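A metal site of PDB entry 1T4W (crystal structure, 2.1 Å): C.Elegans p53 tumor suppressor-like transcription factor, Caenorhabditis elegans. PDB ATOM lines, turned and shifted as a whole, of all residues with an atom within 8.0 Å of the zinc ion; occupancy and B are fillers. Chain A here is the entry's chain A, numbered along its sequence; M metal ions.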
ATOM      1  N   MET A  35     -10.011  17.335   3.999  1.00  0.00           N
ATOM      2  CA  MET A  35     -10.160  16.824   5.359  1.00  0.00           C
ATOM      3  C   MET A  35      -8.769  16.815   6.006  1.00  0.00           C
ATOM      4  O   MET A  35      -7.770  16.908   5.307  1.00  0.00           O
ATOM      5  CB  MET A  35     -10.811  15.419   5.369  1.00  0.00           C
ATOM      6  CG  MET A  35      -9.974  14.287   4.838  1.00  0.00           C
ATOM      7  SD  MET A  35     -10.739  12.653   5.287  1.00  0.00           S
ATOM      8  CE  MET A  35      -9.950  12.353   6.867  1.00  0.00           C
ATOM      9  N   MET A  83     -22.670  12.473   9.873  1.00  0.00           N
ATOM     10  CA  MET A  83     -22.115  11.268  10.497  1.00  0.00           C
ATOM     11  C   MET A  83     -20.812  10.807   9.870  1.00  0.00           C
ATOM     12  O   MET A  83     -20.717  10.656   8.653  1.00  0.00           O
ATOM     13  CB  MET A  83     -23.127  10.135  10.424  1.00  0.00           C
ATOM     14  CG  MET A  83     -24.495  10.461  11.002  1.00  0.00           C
ATOM     15  SD  MET A  83     -24.407  11.031  12.720  1.00  0.00           S
ATOM     16  CE  MET A  83     -23.908   9.541  13.584  1.00  0.00           C
ATOM     17  N   LYS A  84     -19.839  10.555  10.719  1.00  0.00           N
ATOM     18  CA  LYS A  84     -18.517  10.101  10.313  1.00  0.00           C
ATOM     19  C   LYS A  84     -18.644   8.687   9.732  1.00  0.00           C
ATOM     20  O   LYS A  84     -19.437   7.898  10.234  1.00  0.00           O
ATOM     21  CB  LYS A  84     -17.635  10.093  11.557  1.00  0.00           C
ATOM     22  CG  LYS A  84     -16.157  10.152  11.309  1.00  0.00           C
ATOM     23  CD  LYS A  84     -15.461  10.263  12.642  1.00  0.00           C
ATOM     24  CE  LYS A  84     -13.991  10.451  12.497  1.00  0.00           C
ATOM     25  NZ  LYS A  84     -13.477  10.836  13.842  1.00  0.00           N
ATOM     26  N   CYS A  85     -17.895   8.342   8.681  1.00  0.00           N
ATOM     27  CA  CYS A  85     -18.015   6.985   8.134  1.00  0.00           C
ATOM     28  C   CYS A  85     -17.353   5.971   9.065  1.00  0.00           C
ATOM     29  O   CYS A  85     -16.579   6.335   9.973  1.00  0.00           O
ATOM     30  CB  CYS A  85     -17.416   6.875   6.736  1.00  0.00           C
ATOM     31  SG  CYS A  85     -15.617   6.878   6.656  1.00  0.00           S
ATOM     32  N   ARG A  86     -17.648   4.705   8.822  1.00  0.00           N
ATOM     33  CA  ARG A  86     -17.134   3.635   9.648  1.00  0.00           C
ATOM     34  C   ARG A  86     -15.632   3.604   9.675  1.00  0.00           C
ATOM     35  O   ARG A  86     -15.040   3.538  10.758  1.00  0.00           O
ATOM     36  CB  ARG A  86     -17.668   2.284   9.142  1.00  0.00           C
ATOM     37  CG  ARG A  86     -17.411   1.087  10.051  1.00  0.00           C
ATOM     38  CD  ARG A  86     -17.498  -0.235   9.241  1.00  0.00           C
ATOM     39  NE  ARG A  86     -16.303  -0.368   8.404  1.00  0.00           N
ATOM     40  CZ  ARG A  86     -15.075  -0.530   8.872  1.00  0.00           C
ATOM     41  NH1 ARG A  86     -14.876  -0.608  10.187  1.00  0.00           N
ATOM     42  NH2 ARG A  86     -14.020  -0.570   8.052  1.00  0.00           N
ATOM     43  N   SER A  87     -14.985   3.673   8.514  1.00  0.00           N
ATOM     44  CA  SER A  87     -13.525   3.595   8.488  1.00  0.00           C
ATOM     45  C   SER A  87     -12.796   4.770   9.110  1.00  0.00           C
ATOM     46  O   SER A  87     -11.715   4.598   9.687  1.00  0.00           O
ATOM     47  CB  SER A  87     -13.009   3.390   7.063  1.00  0.00           C
ATOM     48  OG  SER A  87     -13.213   4.533   6.273  1.00  0.00           O
ATOM     49  N   HIS A  88     -13.347   5.985   9.004  1.00  0.00           N
ATOM     50  CA  HIS A  88     -12.647   7.107   9.632  1.00  0.00           C
ATOM     51  C   HIS A  88     -12.913   7.068  11.128  1.00  0.00           C
ATOM     52  O   HIS A  88     -12.079   7.507  11.918  1.00  0.00           O
ATOM     53  CB  HIS A  88     -13.069   8.434   9.014  1.00  0.00           C
ATOM     54  CG  HIS A  88     -12.358   8.750   7.730  1.00  0.00           C
ATOM     55  ND1 HIS A  88     -13.008   9.085   6.574  1.00  0.00           N
ATOM     56  CD2 HIS A  88     -11.034   8.732   7.431  1.00  0.00           C
ATOM     57  CE1 HIS A  88     -12.127   9.262   5.603  1.00  0.00           C
ATOM     58  NE2 HIS A  88     -10.926   9.054   6.098  1.00  0.00           N
ATOM     59  N   THR A  89     -14.061   6.532  11.525  1.00  0.00           N
ATOM     60  CA  THR A  89     -14.391   6.431  12.936  1.00  0.00           C
ATOM     61  C   THR A  89     -13.369   5.547  13.642  1.00  0.00           C
ATOM     62  O   THR A  89     -12.665   5.992  14.549  1.00  0.00           O
ATOM     63  CB  THR A  89     -15.785   5.812  13.153  1.00  0.00           C
ATOM     64  OG1 THR A  89     -16.800   6.750  12.785  1.00  0.00           O
ATOM     65  CG2 THR A  89     -15.960   5.433  14.626  1.00  0.00           C
ATOM     66  N   ARG A  91     -10.542   4.502  12.646  1.00  0.00           N
ATOM     67  CA  ARG A  91      -9.170   4.929  12.391  1.00  0.00           C
ATOM     68  C   ARG A  91      -8.840   6.231  13.157  1.00  0.00           C
ATOM     69  O   ARG A  91      -7.704   6.719  13.119  1.00  0.00           O
ATOM     70  CB  ARG A  91      -8.991   5.130  10.881  1.00  0.00           C
ATOM     71  CG  ARG A  91      -7.861   6.045  10.462  1.00  0.00           C
ATOM     72  CD  ARG A  91      -7.857   6.245   8.958  1.00  0.00           C
ATOM     73  NE  ARG A  91      -6.842   7.213   8.530  1.00  0.00           N
ATOM     74  CZ  ARG A  91      -6.635   7.573   7.267  1.00  0.00           C
ATOM     75  NH1 ARG A  91      -5.691   8.462   6.978  1.00  0.00           N
ATOM     76  NH2 ARG A  91      -7.374   7.052   6.290  1.00  0.00           N
ATOM     77  N   PHE A 100     -17.401  13.886  13.708  1.00  0.00           N
ATOM     78  CA  PHE A 100     -17.006  14.212  12.355  1.00  0.00           C
ATOM     79  C   PHE A 100     -15.927  15.319  12.353  1.00  0.00           C
ATOM     80  O   PHE A 100     -15.027  15.339  11.496  1.00  0.00           O
ATOM     81  CB  PHE A 100     -18.239  14.674  11.564  1.00  0.00           C
ATOM     82  CG  PHE A 100     -18.066  14.617  10.062  1.00  0.00           C
ATOM     83  CD1 PHE A 100     -17.313  15.590   9.384  1.00  0.00           C
ATOM     84  CD2 PHE A 100     -18.620  13.569   9.322  1.00  0.00           C
ATOM     85  CE1 PHE A 100     -17.103  15.512   7.984  1.00  0.00           C
ATOM     86  CE2 PHE A 100     -18.409  13.473   7.930  1.00  0.00           C
ATOM     87  CZ  PHE A 100     -17.645  14.444   7.270  1.00  0.00           C
ATOM     88  N   MET A 138     -12.550  15.294   9.919  1.00  0.00           N
ATOM     89  CA  MET A 138     -11.882  14.017   9.827  1.00  0.00           C
ATOM     90  C   MET A 138     -12.617  12.955   9.011  1.00  0.00           C
ATOM     91  O   MET A 138     -12.444  11.758   9.232  1.00  0.00           O
ATOM     92  CB  MET A 138     -11.539  13.510  11.230  1.00  0.00           C
ATOM     93  CG  MET A 138     -10.531  14.405  11.958  1.00  0.00           C
ATOM     94  SD  MET A 138      -8.996  14.688  11.011  1.00  0.00           S
ATOM     95  CE  MET A 138      -8.245  13.079  11.149  1.00  0.00           C
ATOM     96  N   CYS A 139     -13.431  13.402   8.075  1.00  0.00           N
ATOM     97  CA  CYS A 139     -14.140  12.494   7.181  1.00  0.00           C
ATOM     98  C   CYS A 139     -14.493  13.408   6.027  1.00  0.00           C
ATOM     99  O   CYS A 139     -14.311  14.634   6.119  1.00  0.00           O
ATOM    100  CB  CYS A 139     -15.373  11.893   7.880  1.00  0.00           C
ATOM    101  SG  CYS A 139     -16.358  10.721   6.925  1.00  0.00           S
ATOM    102  N   GLN A 140     -14.954  12.870   4.926  1.00  0.00           N
ATOM    103  CA  GLN A 140     -15.238  13.753   3.816  1.00  0.00           C
ATOM    104  C   GLN A 140     -16.432  13.350   2.974  1.00  0.00           C
ATOM    105  O   GLN A 140     -16.990  12.255   3.139  1.00  0.00           O
ATOM    106  CB  GLN A 140     -13.985  13.878   2.961  1.00  0.00           C
ATOM    107  CG  GLN A 140     -13.587  12.597   2.286  1.00  0.00           C
ATOM    108  CD  GLN A 140     -12.197  12.698   1.713  1.00  0.00           C
ATOM    109  OE1 GLN A 140     -11.818  13.742   1.199  1.00  0.00           O
ATOM    110  NE2 GLN A 140     -11.439  11.615   1.807  1.00  0.00           N
ATOM    111  N   GLU A 141     -16.811  14.237   2.073  1.00  0.00           N
ATOM    112  CA  GLU A 141     -17.939  14.026   1.186  1.00  0.00           C
ATOM    113  C   GLU A 141     -17.836  12.675   0.478  1.00  0.00           C
ATOM    114  O   GLU A 141     -18.811  11.931   0.391  1.00  0.00           O
ATOM    115  CB  GLU A 141     -17.976  15.157   0.151  1.00  0.00           C
ATOM    116  CG  GLU A 141     -19.321  15.358  -0.515  1.00  0.00           C
ATOM    117  CD  GLU A 141     -19.276  16.505  -1.498  1.00  0.00           C
ATOM    118  OE1 GLU A 141     -18.794  16.299  -2.635  1.00  0.00           O
ATOM    119  OE2 GLU A 141     -19.685  17.619  -1.117  1.00  0.00           O
ATOM    120  N   LYS A 142     -16.654  12.369  -0.044  1.00  0.00           N
ATOM    121  CA  LYS A 142     -16.436  11.147  -0.776  1.00  0.00           C
ATOM    122  C   LYS A 142     -16.872   9.891  -0.004  1.00  0.00           C
ATOM    123  O   LYS A 142     -17.310   8.913  -0.598  1.00  0.00           O
ATOM    124  CB  LYS A 142     -14.954  11.041  -1.159  1.00  0.00           C
ATOM    125  CG  LYS A 142     -14.633  10.001  -2.181  1.00  0.00           C
ATOM    126  CD  LYS A 142     -13.146  10.017  -2.534  1.00  0.00           C
ATOM    127  CE  LYS A 142     -12.825   8.994  -3.617  1.00  0.00           C
ATOM    128  NZ  LYS A 142     -11.371   8.944  -3.967  1.00  0.00           N
ATOM    129  N   CYS A 143     -16.783   9.951   1.324  1.00  0.00           N
ATOM    130  CA  CYS A 143     -17.160   8.826   2.189  1.00  0.00           C
ATOM    131  C   CYS A 143     -18.651   8.546   2.327  1.00  0.00           C
ATOM    132  O   CYS A 143     -19.043   7.422   2.651  1.00  0.00           O
ATOM    133  CB  CYS A 143     -16.628   9.057   3.607  1.00  0.00           C
ATOM    134  SG  CYS A 143     -14.873   9.227   3.676  1.00  0.00           S
ATOM    135  N   LEU A 144     -19.475   9.555   2.092  1.00  0.00           N
ATOM    136  CA  LEU A 144     -20.912   9.425   2.291  1.00  0.00           C
ATOM    137  C   LEU A 144     -21.735   8.683   1.242  1.00  0.00           C
ATOM    138  O   LEU A 144     -21.310   8.522   0.097  1.00  0.00           O
ATOM    139  CB  LEU A 144     -21.516  10.804   2.513  1.00  0.00           C
ATOM    140  CG  LEU A 144     -20.790  11.732   3.505  1.00  0.00           C
ATOM    141  CD1 LEU A 144     -21.767  12.815   3.921  1.00  0.00           C
ATOM    142  CD2 LEU A 144     -20.295  10.984   4.743  1.00  0.00           C
HETATM  143 ZN    ZN M   1     -14.900   9.079   6.065  1.00  0.00          ZN
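The zinc ion is bound by ND1 of His 88 (2.0 Å), SG of Cys 139 (2.4 Å), SG of Cys 85 (2.4 Å) and SG of Cys 143 (2.4 Å). The zinc ion has four donor atoms within binding distance.
Residues that only touch the zinc ion: Gln 140 (3.96 Å). Five residues have an atom within 4 Å of the zinc ion: Cys 85, His 88, Cys 139, Gln 140 and Cys 143. The nearest printed residue that does not touch the zinc ion is Met 138 (4.8 Å).
A ring nitrogen (NE2) of His 88 sits close to the side-chain sulfur of Met 35 (3.7 Å). The side-chain hydroxyl (OG) of Ser 87 lies close to the side-chain sulfur (SG) of Cys 85. The backbone carbonyl oxygen (O) of Cys 85 sits at hydrogen-bond distance from the side-chain hydroxyl (OG1) of Thr 89, 2.9 Å away. SG of Cys 143 lies close to O of Gln 140, at 3.7 Å. The side-chain amide nitrogen (NE2) of Gln 140 sits at hydrogen-bond distance from the side-chain sulfur (SD) of Met 35 (3.7 Å).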
